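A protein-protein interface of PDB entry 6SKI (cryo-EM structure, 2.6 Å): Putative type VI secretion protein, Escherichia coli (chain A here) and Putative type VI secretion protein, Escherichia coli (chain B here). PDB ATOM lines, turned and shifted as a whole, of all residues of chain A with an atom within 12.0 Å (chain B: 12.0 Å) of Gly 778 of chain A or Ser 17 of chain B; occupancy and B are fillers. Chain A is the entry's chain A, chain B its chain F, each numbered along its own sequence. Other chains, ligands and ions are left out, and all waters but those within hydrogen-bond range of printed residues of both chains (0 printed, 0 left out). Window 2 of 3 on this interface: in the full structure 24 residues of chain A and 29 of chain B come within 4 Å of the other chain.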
ATOM      1  N   GLY A 778     -20.442 -19.600 -19.880  1.00  0.00           N
ATOM      2  CA  GLY A 778     -21.440 -18.950 -19.052  1.00  0.00           C
ATOM      3  C   GLY A 778     -22.548 -18.274 -19.838  1.00  0.00           C
ATOM      4  O   GLY A 778     -22.628 -18.407 -21.060  1.00  0.00           O
ATOM      5  N   GLY A 779     -23.406 -17.541 -19.131  1.00  0.00           N
ATOM      6  CA  GLY A 779     -24.527 -16.849 -19.723  1.00  0.00           C
ATOM      7  C   GLY A 779     -25.779 -17.077 -18.908  1.00  0.00           C
ATOM      8  O   GLY A 779     -25.722 -17.502 -17.749  1.00  0.00           O
ATOM      9  N   GLY A 780     -26.920 -16.795 -19.522  1.00  0.00           N
ATOM     10  CA  GLY A 780     -28.190 -16.945 -18.836  1.00  0.00           C
ATOM     11  C   GLY A 780     -29.333 -16.566 -19.751  1.00  0.00           C
ATOM     12  O   GLY A 780     -29.144 -16.273 -20.936  1.00  0.00           O
ATOM     13  N   PHE A 781     -30.531 -16.568 -19.176  1.00  0.00           N
ATOM     14  CA  PHE A 781     -31.760 -16.312 -19.910  1.00  0.00           C
ATOM     15  C   PHE A 781     -32.390 -14.995 -19.474  1.00  0.00           C
ATOM     16  O   PHE A 781     -32.071 -14.441 -18.420  1.00  0.00           O
ATOM     17  CB  PHE A 781     -32.771 -17.444 -19.701  1.00  0.00           C
ATOM     18  CG  PHE A 781     -32.278 -18.791 -20.130  1.00  0.00           C
ATOM     19  CD1 PHE A 781     -31.551 -19.585 -19.262  1.00  0.00           C
ATOM     20  CD2 PHE A 781     -32.562 -19.275 -21.392  1.00  0.00           C
ATOM     21  CE1 PHE A 781     -31.106 -20.826 -19.650  1.00  0.00           C
ATOM     22  CE2 PHE A 781     -32.122 -20.514 -21.783  1.00  0.00           C
ATOM     23  CZ  PHE A 781     -31.391 -21.291 -20.912  1.00  0.00           C
ATOM     24  N   ILE A 782     -33.304 -14.505 -20.306  1.00  0.00           N
ATOM     25  CA  ILE A 782     -34.085 -13.309 -20.011  1.00  0.00           C
ATOM     26  C   ILE A 782     -35.525 -13.577 -20.418  1.00  0.00           C
ATOM     27  O   ILE A 782     -35.801 -13.854 -21.588  1.00  0.00           O
ATOM     28  CB  ILE A 782     -33.548 -12.061 -20.739  1.00  0.00           C
ATOM     29  CG1 ILE A 782     -32.120 -11.745 -20.296  1.00  0.00           C
ATOM     30  CG2 ILE A 782     -34.466 -10.868 -20.502  1.00  0.00           C
ATOM     31  CD1 ILE A 782     -31.593 -10.441 -20.847  1.00  0.00           C
ATOM     32  N   LEU A 798     -32.980 -23.667 -14.183  1.00  0.00           N
ATOM     33  CA  LEU A 798     -32.063 -23.861 -15.299  1.00  0.00           C
ATOM     34  C   LEU A 798     -31.264 -25.138 -15.056  1.00  0.00           C
ATOM     35  O   LEU A 798     -30.656 -25.307 -13.993  1.00  0.00           O
ATOM     36  CB  LEU A 798     -31.155 -22.642 -15.481  1.00  0.00           C
ATOM     37  CG  LEU A 798     -29.889 -22.420 -14.647  1.00  0.00           C
ATOM     38  CD1 LEU A 798     -28.676 -23.106 -15.265  1.00  0.00           C
ATOM     39  CD2 LEU A 798     -29.622 -20.939 -14.455  1.00  0.00           C
ATOM     40  N   THR A 799     -31.301 -26.049 -16.025  1.00  0.00           N
ATOM     41  CA  THR A 799     -30.609 -27.327 -15.941  1.00  0.00           C
ATOM     42  C   THR A 799     -29.585 -27.411 -17.063  1.00  0.00           C
ATOM     43  O   THR A 799     -29.885 -27.060 -18.209  1.00  0.00           O
ATOM     44  CB  THR A 799     -31.591 -28.498 -16.035  1.00  0.00           C
ATOM     45  OG1 THR A 799     -32.155 -28.546 -17.351  1.00  0.00           O
ATOM     46  CG2 THR A 799     -32.714 -28.331 -15.023  1.00  0.00           C
ATOM     47  N   THR A 800     -28.382 -27.872 -16.732  1.00  0.00           N
ATOM     48  CA  THR A 800     -27.318 -28.009 -17.721  1.00  0.00           C
ATOM     49  C   THR A 800     -27.368 -29.376 -18.393  1.00  0.00           C
ATOM     50  O   THR A 800     -26.871 -30.363 -17.853  1.00  0.00           O
ATOM     51  CB  THR A 800     -25.932 -27.812 -17.088  1.00  0.00           C
ATOM     52  OG1 THR A 800     -25.491 -29.046 -16.506  1.00  0.00           O
ATOM     53  CG2 THR A 800     -25.991 -26.744 -16.008  1.00  0.00           C
ATOM     54  N   ASP A 804     -26.563 -30.004 -13.783  1.00  0.00           N
ATOM     55  CA  ASP A 804     -26.899 -29.657 -12.407  1.00  0.00           C
ATOM     56  C   ASP A 804     -27.894 -28.499 -12.342  1.00  0.00           C
ATOM     57  O   ASP A 804     -27.882 -27.602 -13.184  1.00  0.00           O
ATOM     58  CB  ASP A 804     -25.622 -29.343 -11.614  1.00  0.00           C
ATOM     59  CG  ASP A 804     -24.764 -28.267 -12.263  1.00  0.00           C
ATOM     60  OD1 ASP A 804     -25.285 -27.188 -12.614  1.00  0.00           O
ATOM     61  OD2 ASP A 804     -23.550 -28.509 -12.424  1.00  0.00           O
ATOM     62  N   LEU A 806     -29.798 -25.207 -11.158  1.00  0.00           N
ATOM     63  CA  LEU A 806     -29.634 -23.893 -10.536  1.00  0.00           C
ATOM     64  C   LEU A 806     -31.005 -23.225 -10.478  1.00  0.00           C
ATOM     65  O   LEU A 806     -31.455 -22.630 -11.462  1.00  0.00           O
ATOM     66  CB  LEU A 806     -28.636 -23.029 -11.304  1.00  0.00           C
ATOM     67  CG  LEU A 806     -27.239 -23.559 -11.620  1.00  0.00           C
ATOM     68  CD1 LEU A 806     -26.316 -22.400 -11.945  1.00  0.00           C
ATOM     69  CD2 LEU A 806     -26.680 -24.356 -10.455  1.00  0.00           C
ATOM     70  N   LYS A 815     -34.227 -11.492 -15.633  1.00  0.00           N
ATOM     71  CA  LYS A 815     -32.963 -12.133 -15.967  1.00  0.00           C
ATOM     72  C   LYS A 815     -32.659 -13.244 -14.974  1.00  0.00           C
ATOM     73  O   LYS A 815     -32.792 -13.059 -13.761  1.00  0.00           O
ATOM     74  CB  LYS A 815     -31.814 -11.122 -15.993  1.00  0.00           C
ATOM     75  CG  LYS A 815     -32.005  -9.987 -16.982  1.00  0.00           C
ATOM     76  CD  LYS A 815     -30.808  -9.042 -17.004  1.00  0.00           C
ATOM     77  CE  LYS A 815     -29.573  -9.672 -16.369  1.00  0.00           C
ATOM     78  NZ  LYS A 815     -28.321  -8.991 -16.786  1.00  0.00           N
ATOM     79  N   THR A 816     -32.257 -14.393 -15.504  1.00  0.00           N
ATOM     80  CA  THR A 816     -31.866 -15.539 -14.705  1.00  0.00           C
ATOM     81  C   THR A 816     -30.554 -15.236 -13.974  1.00  0.00           C
ATOM     82  O   THR A 816     -29.901 -14.217 -14.213  1.00  0.00           O
ATOM     83  CB  THR A 816     -31.745 -16.762 -15.618  1.00  0.00           C
ATOM     84  OG1 THR A 816     -32.929 -16.862 -16.418  1.00  0.00           O
ATOM     85  CG2 THR A 816     -31.630 -18.042 -14.833  1.00  0.00           C
ATOM     86  N   ALA A 817     -30.182 -16.109 -13.039  1.00  0.00           N
ATOM     87  CA  ALA A 817     -28.854 -15.977 -12.459  1.00  0.00           C
ATOM     88  C   ALA A 817     -27.810 -16.509 -13.438  1.00  0.00           C
ATOM     89  O   ALA A 817     -28.084 -17.455 -14.181  1.00  0.00           O
ATOM     90  CB  ALA A 817     -28.758 -16.732 -11.136  1.00  0.00           C
ATOM     91  N   PRO A 818     -26.617 -15.916 -13.472  1.00  0.00           N
ATOM     92  CA  PRO A 818     -25.610 -16.345 -14.450  1.00  0.00           C
ATOM     93  C   PRO A 818     -25.199 -17.794 -14.240  1.00  0.00           C
ATOM     94  O   PRO A 818     -25.137 -18.288 -13.113  1.00  0.00           O
ATOM     95  CB  PRO A 818     -24.442 -15.384 -14.198  1.00  0.00           C
ATOM     96  CG  PRO A 818     -25.042 -14.237 -13.438  1.00  0.00           C
ATOM     97  CD  PRO A 818     -26.098 -14.856 -12.593  1.00  0.00           C
ATOM     98  N   VAL A 819     -24.925 -18.477 -15.347  1.00  0.00           N
ATOM     99  CA  VAL A 819     -24.468 -19.857 -15.299  1.00  0.00           C
ATOM    100  C   VAL A 819     -23.385 -20.094 -16.347  1.00  0.00           C
ATOM    101  O   VAL A 819     -22.286 -20.552 -16.027  1.00  0.00           O
ATOM    102  CB  VAL A 819     -25.629 -20.836 -15.499  1.00  0.00           C
ATOM    103  CG1 VAL A 819     -26.352 -20.536 -16.800  1.00  0.00           C
ATOM    104  CG2 VAL A 819     -25.115 -22.265 -15.488  1.00  0.00           C
ATOM    105  N   VAL A 827     -27.775 -25.093 -21.889  1.00  0.00           N
ATOM    106  CA  VAL A 827     -28.667 -25.177 -20.740  1.00  0.00           C
ATOM    107  C   VAL A 827     -30.099 -24.861 -21.153  1.00  0.00           C
ATOM    108  O   VAL A 827     -30.331 -24.068 -22.063  1.00  0.00           O
ATOM    109  CB  VAL A 827     -28.205 -24.238 -19.613  1.00  0.00           C
ATOM    110  CG1 VAL A 827     -26.832 -24.644 -19.114  1.00  0.00           C
ATOM    111  CG2 VAL A 827     -28.183 -22.798 -20.094  1.00  0.00           C
ATOM    112  N   LYS A 828     -31.059 -25.492 -20.483  1.00  0.00           N
ATOM    113  CA  LYS A 828     -32.473 -25.233 -20.710  1.00  0.00           C
ATOM    114  C   LYS A 828     -33.107 -24.727 -19.424  1.00  0.00           C
ATOM    115  O   LYS A 828     -32.746 -25.163 -18.326  1.00  0.00           O
ATOM    116  CB  LYS A 828     -33.208 -26.483 -21.210  1.00  0.00           C
ATOM    117  CG  LYS A 828     -33.231 -27.643 -20.234  1.00  0.00           C
ATOM    118  CD  LYS A 828     -33.003 -28.961 -20.950  1.00  0.00           C
ATOM    119  CE  LYS A 828     -31.569 -29.083 -21.439  1.00  0.00           C
ATOM    120  NZ  LYS A 828     -30.597 -29.092 -20.313  1.00  0.00           N
ATOM    121  N   THR B  13     -33.929 -22.893 -24.704  1.00  0.00           N
ATOM    122  CA  THR B  13     -32.577 -23.421 -24.601  1.00  0.00           C
ATOM    123  C   THR B  13     -31.584 -22.350 -25.021  1.00  0.00           C
ATOM    124  O   THR B  13     -31.922 -21.407 -25.740  1.00  0.00           O
ATOM    125  CB  THR B  13     -32.391 -24.678 -25.461  1.00  0.00           C
ATOM    126  OG1 THR B  13     -33.021 -24.489 -26.735  1.00  0.00           O
ATOM    127  CG2 THR B  13     -32.999 -25.888 -24.775  1.00  0.00           C
ATOM    128  N   HIS B  14     -30.347 -22.510 -24.559  1.00  0.00           N
ATOM    129  CA  HIS B  14     -29.298 -21.543 -24.843  1.00  0.00           C
ATOM    130  C   HIS B  14     -27.927 -22.193 -24.742  1.00  0.00           C
ATOM    131  O   HIS B  14     -27.765 -23.311 -24.244  1.00  0.00           O
ATOM    132  CB  HIS B  14     -29.379 -20.324 -23.918  1.00  0.00           C
ATOM    133  CG  HIS B  14     -28.662 -19.124 -24.451  1.00  0.00           C
ATOM    134  ND1 HIS B  14     -28.770 -18.714 -25.762  1.00  0.00           N
ATOM    135  CD2 HIS B  14     -27.809 -18.257 -23.855  1.00  0.00           C
ATOM    136  CE1 HIS B  14     -28.012 -17.650 -25.953  1.00  0.00           C
ATOM    137  NE2 HIS B  14     -27.425 -17.346 -24.809  1.00  0.00           N
ATOM    138  N   LYS B  15     -26.937 -21.447 -25.220  1.00  0.00           N
ATOM    139  CA  LYS B  15     -25.557 -21.881 -25.359  1.00  0.00           C
ATOM    140  C   LYS B  15     -24.706 -21.201 -24.295  1.00  0.00           C
ATOM    141  O   LYS B  15     -24.790 -19.982 -24.113  1.00  0.00           O
ATOM    142  CB  LYS B  15     -25.062 -21.538 -26.768  1.00  0.00           C
ATOM    143  CG  LYS B  15     -23.773 -20.733 -26.844  1.00  0.00           C
ATOM    144  CD  LYS B  15     -23.345 -20.505 -28.286  1.00  0.00           C
ATOM    145  CE  LYS B  15     -22.307 -19.398 -28.377  1.00  0.00           C
ATOM    146  NZ  LYS B  15     -21.774 -19.218 -29.754  1.00  0.00           N
ATOM    147  N   THR B  16     -23.927 -21.991 -23.559  1.00  0.00           N
ATOM    148  CA  THR B  16     -22.937 -21.401 -22.671  1.00  0.00           C
ATOM    149  C   THR B  16     -21.627 -21.172 -23.420  1.00  0.00           C
ATOM    150  O   THR B  16     -21.304 -21.858 -24.394  1.00  0.00           O
ATOM    151  CB  THR B  16     -22.699 -22.280 -21.444  1.00  0.00           C
ATOM    152  OG1 THR B  16     -21.677 -23.238 -21.732  1.00  0.00           O
ATOM    153  CG2 THR B  16     -23.975 -23.004 -21.047  1.00  0.00           C
ATOM    154  N   SER B  17     -20.861 -20.193 -22.941  1.00  0.00           N
ATOM    155  CA  SER B  17     -19.673 -19.725 -23.643  1.00  0.00           C
ATOM    156  C   SER B  17     -18.884 -18.755 -22.776  1.00  0.00           C
ATOM    157  O   SER B  17     -19.182 -18.589 -21.590  1.00  0.00           O
ATOM    158  CB  SER B  17     -20.057 -19.061 -24.968  1.00  0.00           C
ATOM    159  OG  SER B  17     -20.965 -17.995 -24.757  1.00  0.00           O
ATOM    160  N   ILE B  18     -17.867 -18.125 -23.355  1.00  0.00           N
ATOM    161  CA  ILE B  18     -17.206 -16.995 -22.718  1.00  0.00           C
ATOM    162  C   ILE B  18     -17.853 -15.670 -23.101  1.00  0.00           C
ATOM    163  O   ILE B  18     -17.518 -14.640 -22.496  1.00  0.00           O
ATOM    164  CB  ILE B  18     -15.697 -16.965 -23.034  1.00  0.00           C
ATOM    165  CG1 ILE B  18     -15.457 -17.196 -24.527  1.00  0.00           C
ATOM    166  CG2 ILE B  18     -14.957 -17.989 -22.187  1.00  0.00           C
ATOM    167  CD1 ILE B  18     -14.304 -16.398 -25.092  1.00  0.00           C
ATOM    168  N   HIS B  19     -18.756 -15.660 -24.086  1.00  0.00           N
ATOM    169  CA  HIS B  19     -19.605 -14.497 -24.314  1.00  0.00           C
ATOM    170  C   HIS B  19     -20.381 -14.132 -23.061  1.00  0.00           C
ATOM    171  O   HIS B  19     -20.573 -12.945 -22.771  1.00  0.00           O
ATOM    172  CB  HIS B  19     -20.601 -14.779 -25.442  1.00  0.00           C
ATOM    173  CG  HIS B  19     -20.034 -14.647 -26.820  1.00  0.00           C
ATOM    174  ND1 HIS B  19     -20.671 -15.155 -27.931  1.00  0.00           N
ATOM    175  CD2 HIS B  19     -18.900 -14.061 -27.271  1.00  0.00           C
ATOM    176  CE1 HIS B  19     -19.954 -14.889 -29.007  1.00  0.00           C
ATOM    177  NE2 HIS B  19     -18.873 -14.228 -28.634  1.00  0.00           N
ATOM    178  N   ASN B  20     -20.823 -15.140 -22.307  1.00  0.00           N
ATOM    179  CA  ASN B  20     -21.727 -14.960 -21.175  1.00  0.00           C
ATOM    180  C   ASN B  20     -22.935 -14.128 -21.593  1.00  0.00           C
ATOM    181  O   ASN B  20     -23.363 -13.203 -20.901  1.00  0.00           O
ATOM    182  CB  ASN B  20     -20.999 -14.340 -19.985  1.00  0.00           C
ATOM    183  CG  ASN B  20     -20.016 -15.301 -19.343  1.00  0.00           C
ATOM    184  OD1 ASN B  20     -20.314 -15.922 -18.324  1.00  0.00           O
ATOM    185  ND2 ASN B  20     -18.836 -15.425 -19.938  1.00  0.00           N
ATOM    186  N   ASP B  21     -23.485 -14.473 -22.755  1.00  0.00           N
ATOM    187  CA  ASP B  21     -24.549 -13.691 -23.362  1.00  0.00           C
ATOM    188  C   ASP B  21     -25.902 -14.042 -22.761  1.00  0.00           C
ATOM    189  O   ASP B  21     -26.201 -15.209 -22.492  1.00  0.00           O
ATOM    190  CB  ASP B  21     -24.577 -13.908 -24.873  1.00  0.00           C
ATOM    191  CG  ASP B  21     -24.788 -12.617 -25.638  1.00  0.00           C
ATOM    192  OD1 ASP B  21     -24.095 -12.405 -26.655  1.00  0.00           O
ATOM    193  OD2 ASP B  21     -25.649 -11.813 -25.220  1.00  0.00           O
ATOM    194  N   TRP B  22     -26.720 -13.013 -22.557  1.00  0.00           N
ATOM    195  CA  TRP B  22     -28.055 -13.156 -21.994  1.00  0.00           C
ATOM    196  C   TRP B  22     -29.066 -13.129 -23.131  1.00  0.00           C
ATOM    197  O   TRP B  22     -29.179 -12.125 -23.843  1.00  0.00           O
ATOM    198  CB  TRP B  22     -28.334 -12.043 -20.989  1.00  0.00           C
ATOM    199  CG  TRP B  22     -27.408 -12.081 -19.833  1.00  0.00           C
ATOM    200  CD1 TRP B  22     -26.192 -11.475 -19.737  1.00  0.00           C
ATOM    201  CD2 TRP B  22     -27.607 -12.778 -18.604  1.00  0.00           C
ATOM    202  NE1 TRP B  22     -25.623 -11.745 -18.519  1.00  0.00           N
ATOM    203  CE2 TRP B  22     -26.474 -12.544 -17.804  1.00  0.00           C
ATOM    204  CE3 TRP B  22     -28.637 -13.574 -18.101  1.00  0.00           C
ATOM    205  CZ2 TRP B  22     -26.342 -13.077 -16.528  1.00  0.00           C
ATOM    206  CZ3 TRP B  22     -28.503 -14.103 -16.839  1.00  0.00           C
ATOM    207  CH2 TRP B  22     -27.366 -13.851 -16.064  1.00  0.00           C
ATOM    208  N   LYS B  23     -29.795 -14.227 -23.298  1.00  0.00           N
ATOM    209  CA  LYS B  23     -30.689 -14.416 -24.433  1.00  0.00           C
ATOM    210  C   LYS B  23     -32.130 -14.263 -23.983  1.00  0.00           C
ATOM    211  O   LYS B  23     -32.554 -14.909 -23.020  1.00  0.00           O
ATOM    212  CB  LYS B  23     -30.493 -15.793 -25.062  1.00  0.00           C
ATOM    213  N   VAL B  24     -32.878 -13.411 -24.686  1.00  0.00           N
ATOM    214  CA  VAL B  24     -34.287 -13.235 -24.369  1.00  0.00           C
ATOM    215  C   VAL B  24     -35.023 -14.551 -24.573  1.00  0.00           C
ATOM    216  O   VAL B  24     -34.706 -15.339 -25.475  1.00  0.00           O
ATOM    217  CB  VAL B  24     -34.907 -12.103 -25.208  1.00  0.00           C
ATOM    218  CG1 VAL B  24     -35.356 -12.606 -26.574  1.00  0.00           C
ATOM    219  CG2 VAL B  24     -36.080 -11.483 -24.471  1.00  0.00           C
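N of His 14 of chain B sits at hydrogen-bond distance from O of Val 827 of chain A, at 2.9 Å.
N of Ser 17 of chain B is in hydrogen-bond range of O of Gly 778 of chain A, at 3.1 Å.
O of Asp 21 of chain B lies within hydrogen-bond range of N of Gly 780 of chain A, at 3.4 Å.
The backbone carbonyl oxygen of Gly 780 of chain A is in hydrogen-bond range of the backbone NH of Lys 23 of chain B, 3.2 Å away.
The backbone carbonyl oxygen of Lys 23 of chain B lies within hydrogen-bond range of the backbone NH of Ile 782 of chain A.
Hydrophobic or aromatic side chains of chain B that line the printed part of chain A: His 14, Trp 22 and Val 24.
Printed residues of chain A that touch a printed residue of chain B: Gly 778, Gly 779, Gly 780, Phe 781, Ile 782, Thr 816, Ala 817, Pro 818, Val 827 and Lys 828.
Hydrophobic or aromatic side chains of chain A within 4 Å of the printed part of chain B: Phe 781, Ile 782, Pro 818 and Val 827.
Among the printed residues, 23 pairs touch across the chains.
Among the printed residues, no Asp or Glu carboxylate lies within 4 Å of a Lys or Arg side-chain nitrogen of the other chain.
Among the printed residues, merely in contact across the chains: Thr 816 of chain A with Trp 22 of chain B (3.0 Å), Ile 782 of chain A with Val 24 of chain B (3.2 Å), Gly 778 of chain A with Asn 20 of chain B (3.3 Å), Pro 818 of chain A with Trp 22 of chain B (3.4 Å), Gly 778 of chain A with Thr 16 of chain B (3.4 Å), Val 827 of chain A with Thr 13 of chain B (3.5 Å), Gly 780 of chain A with Trp 22 of chain B (3.5 Å), Phe 781 of chain A with His 14 of chain B (3.5 Å), Phe 781 of chain A with Lys 23 of chain B (3.5 Å), Phe 781 of chain A with Trp 22 of chain B (3.6 Å), Gly 779 of chain A with Asn 20 of chain B (3.6 Å), Lys 828 of chain A with Thr 13 of chain B (3.6 Å), Gly 779 of chain A with Asp 21 of chain B (3.6 Å), Ile 782 of chain A with Trp 22 of chain B (3.6 Å), Phe 781 of chain A with Thr 13 of chain B (3.8 Å), Ala 817 of chain A with Trp 22 of chain B (3.8 Å), Gly 780 of chain A with His 14 of chain B (3.8 Å) and Val 827 of chain A with Thr 16 of chain B (3.8 Å).
Of chain B, only Thr 16 (3.4 Å), Ser 17 (2.4 Å) and Asn 20 (3.3 Å) come within 4 Å of Gly 778 of chain A.
Printed residues of chain B within 4 Å of Gly 779 of chain A: Asn 20 (3.6 Å) and Asp 21 (3.6 Å).
No residue of chain B comes within 4 Å of Val 819 of chain A.
No residue of chain A comes within 4 Å of Lys 15 of chain B.
No residue of chain A comes within 4 Å of His 19 of chain B.
Asn 20 of chain B touches just these residues of chain A: Gly 778 and Gly 779.
Asp 21 of chain B touches two residues of chain A.
Of the printed residues of chain B, Lys 828 of chain A touches Thr 13.
Of the printed residues of chain B, Pro 818 of chain A touches Trp 22 (3.4 Å).
The nearest printed residue of chain A that does not touch Thr 13 of chain B is Thr 799 of chain A (7.4 Å).
The backbone carbonyl oxygen (O) of Asp 21 of chain B is in hydrogen-bond range of a ring nitrogen (NE2) of His 14 of chain B, at 3.4 Å.
The side-chain hydroxyl of Ser 17 of chain B lies within hydrogen-bond range of the backbone NH of His 19 of chain B, at 3.3 Å.
The backbone carbonyl oxygen of Ile 18 of chain B sits at hydrogen-bond distance from the side-chain amide nitrogen of Asn 20 of chain B (3.0 Å).
O of Gly 779 of chain A is in hydrogen-bond range of N of Val 819 of chain A, at 2.7 Å.
The backbone NH of Thr 816 of chain A sits at hydrogen-bond distance from the backbone carbonyl oxygen of Phe 781 of chain A, 2.9 Å away.
The backbone NH (N) of Thr 799 of chain A sits at hydrogen-bond distance from the backbone carbonyl oxygen (O) of Lys 828 of chain A (2.9 Å).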
